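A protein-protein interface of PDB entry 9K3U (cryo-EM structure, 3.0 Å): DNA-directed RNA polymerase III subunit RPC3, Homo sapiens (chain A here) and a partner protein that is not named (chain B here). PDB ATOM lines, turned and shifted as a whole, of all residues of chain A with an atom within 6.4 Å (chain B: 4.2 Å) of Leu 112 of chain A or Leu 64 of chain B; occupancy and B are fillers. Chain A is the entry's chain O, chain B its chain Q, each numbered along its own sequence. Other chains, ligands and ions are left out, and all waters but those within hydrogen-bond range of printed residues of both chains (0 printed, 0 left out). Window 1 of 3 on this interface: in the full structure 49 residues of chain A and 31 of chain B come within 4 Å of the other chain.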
ATOM      1  N   PHE A  17     -24.753 -13.320   3.295  1.00  0.00           N
ATOM      2  CA  PHE A  17     -25.623 -14.269   3.983  1.00  0.00           C
ATOM      3  C   PHE A  17     -24.900 -15.130   5.006  1.00  0.00           C
ATOM      4  O   PHE A  17     -25.399 -15.291   6.124  1.00  0.00           O
ATOM      5  CB  PHE A  17     -26.318 -15.180   2.960  1.00  0.00           C
ATOM      6  CG  PHE A  17     -27.144 -14.438   1.945  1.00  0.00           C
ATOM      7  CD1 PHE A  17     -27.805 -13.269   2.283  1.00  0.00           C
ATOM      8  CD2 PHE A  17     -27.261 -14.914   0.650  1.00  0.00           C
ATOM      9  CE1 PHE A  17     -28.567 -12.589   1.349  1.00  0.00           C
ATOM     10  CE2 PHE A  17     -28.019 -14.239  -0.287  1.00  0.00           C
ATOM     11  CZ  PHE A  17     -28.673 -13.076   0.063  1.00  0.00           C
ATOM     12  N   HIS A  60     -34.671 -15.109  -1.879  1.00  0.00           N
ATOM     13  CA  HIS A  60     -34.130 -13.976  -2.617  1.00  0.00           C
ATOM     14  C   HIS A  60     -34.149 -14.196  -4.128  1.00  0.00           C
ATOM     15  O   HIS A  60     -33.509 -13.436  -4.863  1.00  0.00           O
ATOM     16  CB  HIS A  60     -32.702 -13.682  -2.151  1.00  0.00           C
ATOM     17  CG  HIS A  60     -32.613 -13.240  -0.724  1.00  0.00           C
ATOM     18  ND1 HIS A  60     -32.969 -14.051   0.331  1.00  0.00           N
ATOM     19  CD2 HIS A  60     -32.205 -12.070  -0.176  1.00  0.00           C
ATOM     20  CE1 HIS A  60     -32.787 -13.402   1.465  1.00  0.00           C
ATOM     21  NE2 HIS A  60     -32.323 -12.197   1.188  1.00  0.00           N
ATOM     22  N   TYR A  88     -27.278  -3.643  -6.324  1.00  0.00           N
ATOM     23  CA  TYR A  88     -28.296  -3.068  -5.446  1.00  0.00           C
ATOM     24  C   TYR A  88     -28.035  -1.598  -5.149  1.00  0.00           C
ATOM     25  O   TYR A  88     -28.980  -0.795  -5.249  1.00  0.00           O
ATOM     26  CB  TYR A  88     -28.390  -3.886  -4.157  1.00  0.00           C
ATOM     27  CG  TYR A  88     -28.981  -5.275  -4.321  1.00  0.00           C
ATOM     28  CD1 TYR A  88     -29.564  -5.676  -5.521  1.00  0.00           C
ATOM     29  CD2 TYR A  88     -28.962  -6.182  -3.270  1.00  0.00           C
ATOM     30  CE1 TYR A  88     -30.102  -6.941  -5.664  1.00  0.00           C
ATOM     31  CE2 TYR A  88     -29.499  -7.447  -3.407  1.00  0.00           C
ATOM     32  CZ  TYR A  88     -30.068  -7.821  -4.605  1.00  0.00           C
ATOM     33  OH  TYR A  88     -30.604  -9.080  -4.744  1.00  0.00           O
ATOM     34  N   PRO A  89     -26.819  -1.172  -4.786  1.00  0.00           N
ATOM     35  CA  PRO A  89     -26.609   0.264  -4.537  1.00  0.00           C
ATOM     36  C   PRO A  89     -27.016   1.137  -5.711  1.00  0.00           C
ATOM     37  O   PRO A  89     -27.635   2.190  -5.513  1.00  0.00           O
ATOM     38  CB  PRO A  89     -25.104   0.352  -4.252  1.00  0.00           C
ATOM     39  CG  PRO A  89     -24.720  -1.010  -3.794  1.00  0.00           C
ATOM     40  CD  PRO A  89     -25.594  -1.956  -4.556  1.00  0.00           C
ATOM     41  N   ILE A  92     -30.812   1.388  -5.792  1.00  0.00           N
ATOM     42  CA  ILE A  92     -31.322   2.314  -4.786  1.00  0.00           C
ATOM     43  C   ILE A  92     -31.066   3.751  -5.215  1.00  0.00           C
ATOM     44  O   ILE A  92     -31.929   4.624  -5.066  1.00  0.00           O
ATOM     45  CB  ILE A  92     -30.692   2.013  -3.411  1.00  0.00           C
ATOM     46  CG1 ILE A  92     -30.959   0.560  -3.001  1.00  0.00           C
ATOM     47  CG2 ILE A  92     -31.229   2.969  -2.359  1.00  0.00           C
ATOM     48  CD1 ILE A  92     -32.427   0.191  -2.916  1.00  0.00           C
ATOM     49  N   VAL A 107     -37.924  -0.014  -2.553  1.00  0.00           N
ATOM     50  CA  VAL A 107     -36.988  -0.825  -3.327  1.00  0.00           C
ATOM     51  C   VAL A 107     -35.948  -1.455  -2.412  1.00  0.00           C
ATOM     52  O   VAL A 107     -35.539  -2.605  -2.611  1.00  0.00           O
ATOM     53  CB  VAL A 107     -36.331   0.023  -4.430  1.00  0.00           C
ATOM     54  CG1 VAL A 107     -35.336  -0.812  -5.227  1.00  0.00           C
ATOM     55  CG2 VAL A 107     -37.391   0.618  -5.350  1.00  0.00           C
ATOM     56  N   GLU A 108     -35.503  -0.716  -1.394  1.00  0.00           N
ATOM     57  CA  GLU A 108     -34.519  -1.260  -0.462  1.00  0.00           C
ATOM     58  C   GLU A 108     -35.072  -2.478   0.263  1.00  0.00           C
ATOM     59  O   GLU A 108     -34.415  -3.523   0.340  1.00  0.00           O
ATOM     60  CB  GLU A 108     -34.094  -0.179   0.534  1.00  0.00           C
ATOM     61  CG  GLU A 108     -33.018  -0.625   1.513  1.00  0.00           C
ATOM     62  CD  GLU A 108     -32.580   0.490   2.445  1.00  0.00           C
ATOM     63  OE1 GLU A 108     -33.099   1.618   2.308  1.00  0.00           O
ATOM     64  OE2 GLU A 108     -31.718   0.238   3.311  1.00  0.00           O
ATOM     65  N   GLU A 109     -36.284  -2.360   0.807  1.00  0.00           N
ATOM     66  CA  GLU A 109     -36.895  -3.487   1.504  1.00  0.00           C
ATOM     67  C   GLU A 109     -37.119  -4.660   0.560  1.00  0.00           C
ATOM     68  O   GLU A 109     -36.889  -5.816   0.936  1.00  0.00           O
ATOM     69  CB  GLU A 109     -38.215  -3.054   2.143  1.00  0.00           C
ATOM     70  CG  GLU A 109     -38.062  -2.034   3.259  1.00  0.00           C
ATOM     71  CD  GLU A 109     -37.332  -2.592   4.466  1.00  0.00           C
ATOM     72  OE1 GLU A 109     -37.108  -3.821   4.513  1.00  0.00           O
ATOM     73  OE2 GLU A 109     -36.980  -1.802   5.367  1.00  0.00           O
ATOM     74  N   LEU A 110     -37.565  -4.388  -0.668  1.00  0.00           N
ATOM     75  CA  LEU A 110     -37.769  -5.473  -1.625  1.00  0.00           C
ATOM     76  C   LEU A 110     -36.465  -6.208  -1.908  1.00  0.00           C
ATOM     77  O   LEU A 110     -36.427  -7.442  -1.890  1.00  0.00           O
ATOM     78  CB  LEU A 110     -38.369  -4.928  -2.922  1.00  0.00           C
ATOM     79  CG  LEU A 110     -39.897  -4.949  -3.048  1.00  0.00           C
ATOM     80  CD1 LEU A 110     -40.436  -6.367  -2.921  1.00  0.00           C
ATOM     81  CD2 LEU A 110     -40.553  -4.034  -2.024  1.00  0.00           C
ATOM     82  N   LEU A 111     -35.384  -5.467  -2.157  1.00  0.00           N
ATOM     83  CA  LEU A 111     -34.106  -6.099  -2.461  1.00  0.00           C
ATOM     84  C   LEU A 111     -33.515  -6.818  -1.254  1.00  0.00           C
ATOM     85  O   LEU A 111     -32.798  -7.812  -1.424  1.00  0.00           O
ATOM     86  CB  LEU A 111     -33.111  -5.057  -2.980  1.00  0.00           C
ATOM     87  CG  LEU A 111     -33.461  -4.388  -4.312  1.00  0.00           C
ATOM     88  CD1 LEU A 111     -32.434  -3.320  -4.655  1.00  0.00           C
ATOM     89  CD2 LEU A 111     -33.563  -5.414  -5.431  1.00  0.00           C
ATOM     90  N   LEU A 112     -33.797  -6.340  -0.041  1.00  0.00           N
ATOM     91  CA  LEU A 112     -33.238  -6.966   1.152  1.00  0.00           C
ATOM     92  C   LEU A 112     -34.039  -8.171   1.624  1.00  0.00           C
ATOM     93  O   LEU A 112     -33.477  -9.044   2.294  1.00  0.00           O
ATOM     94  CB  LEU A 112     -33.140  -5.945   2.287  1.00  0.00           C
ATOM     95  CG  LEU A 112     -31.813  -5.192   2.398  1.00  0.00           C
ATOM     96  CD1 LEU A 112     -31.514  -4.397   1.135  1.00  0.00           C
ATOM     97  CD2 LEU A 112     -31.829  -4.279   3.618  1.00  0.00           C
ATOM     98  N   ASN A 113     -35.331  -8.246   1.290  1.00  0.00           N
ATOM     99  CA  ASN A 113     -36.168  -9.353   1.732  1.00  0.00           C
ATOM    100  C   ASN A 113     -36.499 -10.355   0.637  1.00  0.00           C
ATOM    101  O   ASN A 113     -37.023 -11.428   0.950  1.00  0.00           O
ATOM    102  CB  ASN A 113     -37.481  -8.820   2.322  1.00  0.00           C
ATOM    103  CG  ASN A 113     -37.261  -7.972   3.561  1.00  0.00           C
ATOM    104  OD1 ASN A 113     -37.258  -8.480   4.683  1.00  0.00           O
ATOM    105  ND2 ASN A 113     -37.075  -6.672   3.362  1.00  0.00           N
ATOM    106  N   GLY A 114     -36.211 -10.043  -0.623  1.00  0.00           N
ATOM    107  CA  GLY A 114     -36.476 -10.974  -1.702  1.00  0.00           C
ATOM    108  C   GLY A 114     -37.926 -10.973  -2.139  1.00  0.00           C
ATOM    109  O   GLY A 114     -38.253 -10.488  -3.225  1.00  0.00           O
ATOM    110  N   ARG A 128     -39.986   2.852   9.079  1.00  0.00           N
ATOM    111  CA  ARG A 128     -38.657   3.427   8.911  1.00  0.00           C
ATOM    112  C   ARG A 128     -38.704   4.935   8.698  1.00  0.00           C
ATOM    113  O   ARG A 128     -37.790   5.644   9.133  1.00  0.00           O
ATOM    114  CB  ARG A 128     -37.934   2.757   7.741  1.00  0.00           C
ATOM    115  CG  ARG A 128     -37.562   1.305   8.002  1.00  0.00           C
ATOM    116  CD  ARG A 128     -36.587   0.778   6.960  1.00  0.00           C
ATOM    117  NE  ARG A 128     -35.302   1.473   7.010  1.00  0.00           N
ATOM    118  CZ  ARG A 128     -34.258   1.171   6.247  1.00  0.00           C
ATOM    119  NH1 ARG A 128     -34.334   0.181   5.364  1.00  0.00           N
ATOM    120  NH2 ARG A 128     -33.130   1.859   6.363  1.00  0.00           N
ATOM    121  N   LEU B  60     -24.678   3.999   1.211  1.00  0.00           N
ATOM    122  CA  LEU B  60     -25.762   3.026   1.200  1.00  0.00           C
ATOM    123  C   LEU B  60     -25.223   1.602   1.156  1.00  0.00           C
ATOM    124  O   LEU B  60     -25.767   0.708   1.812  1.00  0.00           O
ATOM    125  CB  LEU B  60     -26.686   3.284   0.011  1.00  0.00           C
ATOM    126  CG  LEU B  60     -27.976   2.462  -0.005  1.00  0.00           C
ATOM    127  CD1 LEU B  60     -29.186   3.359   0.197  1.00  0.00           C
ATOM    128  CD2 LEU B  60     -28.093   1.672  -1.297  1.00  0.00           C
ATOM    129  N   LYS B  61     -24.154   1.372   0.390  1.00  0.00           N
ATOM    130  CA  LYS B  61     -23.558   0.040   0.357  1.00  0.00           C
ATOM    131  C   LYS B  61     -22.982  -0.332   1.717  1.00  0.00           C
ATOM    132  O   LYS B  61     -23.097  -1.484   2.154  1.00  0.00           O
ATOM    133  CB  LYS B  61     -22.479  -0.026  -0.724  1.00  0.00           C
ATOM    134  CG  LYS B  61     -21.976  -1.433  -1.003  1.00  0.00           C
ATOM    135  CD  LYS B  61     -21.025  -1.460  -2.190  1.00  0.00           C
ATOM    136  CE  LYS B  61     -20.577  -2.877  -2.514  1.00  0.00           C
ATOM    137  NZ  LYS B  61     -21.714  -3.746  -2.930  1.00  0.00           N
ATOM    138  N   GLN B  62     -22.366   0.630   2.408  1.00  0.00           N
ATOM    139  CA  GLN B  62     -21.865   0.358   3.752  1.00  0.00           C
ATOM    140  C   GLN B  62     -23.008   0.052   4.714  1.00  0.00           C
ATOM    141  O   GLN B  62     -22.915  -0.876   5.528  1.00  0.00           O
ATOM    142  CB  GLN B  62     -21.043   1.544   4.256  1.00  0.00           C
ATOM    143  CG  GLN B  62     -19.734   1.749   3.510  1.00  0.00           C
ATOM    144  CD  GLN B  62     -18.935   2.923   4.043  1.00  0.00           C
ATOM    145  OE1 GLN B  62     -19.382   3.635   4.943  1.00  0.00           O
ATOM    146  NE2 GLN B  62     -17.746   3.130   3.490  1.00  0.00           N
ATOM    147  N   GLU B  63     -24.095   0.824   4.637  1.00  0.00           N
ATOM    148  CA  GLU B  63     -25.249   0.557   5.488  1.00  0.00           C
ATOM    149  C   GLU B  63     -25.827  -0.825   5.211  1.00  0.00           C
ATOM    150  O   GLU B  63     -26.244  -1.530   6.135  1.00  0.00           O
ATOM    151  CB  GLU B  63     -26.312   1.635   5.283  1.00  0.00           C
ATOM    152  CG  GLU B  63     -25.925   2.999   5.828  1.00  0.00           C
ATOM    153  CD  GLU B  63     -26.975   4.058   5.551  1.00  0.00           C
ATOM    154  OE1 GLU B  63     -28.010   3.725   4.936  1.00  0.00           O
ATOM    155  OE2 GLU B  63     -26.767   5.222   5.952  1.00  0.00           O
ATOM    156  N   LEU B  64     -25.864  -1.229   3.938  1.00  0.00           N
ATOM    157  CA  LEU B  64     -26.348  -2.564   3.605  1.00  0.00           C
ATOM    158  C   LEU B  64     -25.428  -3.637   4.172  1.00  0.00           C
ATOM    159  O   LEU B  64     -25.900  -4.631   4.737  1.00  0.00           O
ATOM    160  CB  LEU B  64     -26.475  -2.714   2.089  1.00  0.00           C
ATOM    161  CG  LEU B  64     -27.585  -1.907   1.412  1.00  0.00           C
ATOM    162  CD1 LEU B  64     -27.575  -2.141  -0.092  1.00  0.00           C
ATOM    163  CD2 LEU B  64     -28.945  -2.251   2.000  1.00  0.00           C
ATOM    164  N   ARG B  65     -24.113  -3.461   4.024  1.00  0.00           N
ATOM    165  CA  ARG B  65     -23.174  -4.409   4.617  1.00  0.00           C
ATOM    166  C   ARG B  65     -23.396  -4.529   6.119  1.00  0.00           C
ATOM    167  O   ARG B  65     -23.316  -5.629   6.682  1.00  0.00           O
ATOM    168  CB  ARG B  65     -21.735  -3.981   4.333  1.00  0.00           C
ATOM    169  CG  ARG B  65     -21.200  -4.393   2.975  1.00  0.00           C
ATOM    170  CD  ARG B  65     -19.679  -4.335   2.962  1.00  0.00           C
ATOM    171  NE  ARG B  65     -19.108  -4.758   1.684  1.00  0.00           N
ATOM    172  CZ  ARG B  65     -18.823  -3.940   0.672  1.00  0.00           C
ATOM    173  NH1 ARG B  65     -19.056  -2.636   0.769  1.00  0.00           N
ATOM    174  NH2 ARG B  65     -18.303  -4.429  -0.443  1.00  0.00           N
ATOM    175  N   GLU B  66     -23.677  -3.407   6.785  1.00  0.00           N
ATOM    176  CA  GLU B  66     -23.829  -3.427   8.237  1.00  0.00           C
ATOM    177  C   GLU B  66     -25.168  -4.009   8.675  1.00  0.00           C
ATOM    178  O   GLU B  66     -25.246  -4.622   9.745  1.00  0.00           O
ATOM    179  CB  GLU B  66     -23.672  -2.012   8.797  1.00  0.00           C
ATOM    180  CG  GLU B  66     -22.268  -1.445   8.660  1.00  0.00           C
ATOM    181  CD  GLU B  66     -22.156  -0.032   9.202  1.00  0.00           C
ATOM    182  OE1 GLU B  66     -23.178   0.503   9.685  1.00  0.00           O
ATOM    183  OE2 GLU B  66     -21.047   0.539   9.148  1.00  0.00           O
ATOM    184  N   THR B  67     -26.221  -3.833   7.877  1.00  0.00           N
ATOM    185  CA  THR B  67     -27.560  -4.247   8.280  1.00  0.00           C
ATOM    186  C   THR B  67     -27.951  -5.634   7.784  1.00  0.00           C
ATOM    187  O   THR B  67     -28.896  -6.219   8.323  1.00  0.00           O
ATOM    188  CB  THR B  67     -28.602  -3.240   7.781  1.00  0.00           C
ATOM    189  OG1 THR B  67     -29.868  -3.508   8.399  1.00  0.00           O
ATOM    190  CG2 THR B  67     -28.754  -3.334   6.270  1.00  0.00           C
ATOM    191  N   MET B  68     -27.259  -6.175   6.778  1.00  0.00           N
ATOM    192  CA  MET B  68     -27.614  -7.481   6.243  1.00  0.00           C
ATOM    193  C   MET B  68     -27.014  -8.635   7.034  1.00  0.00           C
ATOM    194  O   MET B  68     -27.531  -9.755   6.953  1.00  0.00           O
ATOM    195  CB  MET B  68     -27.174  -7.583   4.778  1.00  0.00           C
ATOM    196  CG  MET B  68     -27.489  -8.918   4.122  1.00  0.00           C
ATOM    197  SD  MET B  68     -27.418  -8.839   2.322  1.00  0.00           S
ATOM    198  CE  MET B  68     -25.809  -8.094   2.070  1.00  0.00           C
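The side-chain carboxylate of Glu 108 of chain A lies within salt-bridge range of the guanidinium group of Arg 128 of chain A (3.3 Å).
CD2 of Leu 60 of chain B touches CA of Pro 89 of chain A, 3.8 Å away. Pro 89 of chain A touches Lys 61 of chain B. Leu 60 of chain B touches Ile 92 of chain A. Glu 108 of chain A touches Leu 64 of chain B. Leu 112 of chain A touches Leu 64 of chain B.
Of chain B, only Leu 64 comes within 4 Å of Leu 112 of chain A. Of the printed residues of chain B, Ile 92 of chain A touches Leu 60. Of the printed residues of chain B, Glu 108 of chain A touches Leu 64. Of the printed residues of chain A, Lys 61 of chain B touches Pro 89 (3.9 Å). Of the printed residues of chain B, Pro 89 of chain A touches Leu 60 (3.8 Å) and Lys 61 (3.9 Å). Printed residues of chain A within 4 Å of Leu 60 of chain B: Pro 89 and Ile 92. Gln 62 of chain B touches none of the printed residues of chain A. Tyr 88 of chain A touches none of the printed residues of chain B. The nearest residue of chain A that does not touch Leu 64 of chain B is Tyr 88 of chain A (4.5 Å).
Printed residues of chain A that touch a printed residue of chain B: Pro 89, Ile 92, Glu 108 and Leu 112. Among the printed residues, 5 pairs touch across the chains. Among the printed residues, no Asp or Glu carboxylate lies within 4 Å of a Lys or Arg side-chain nitrogen of the other chain.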
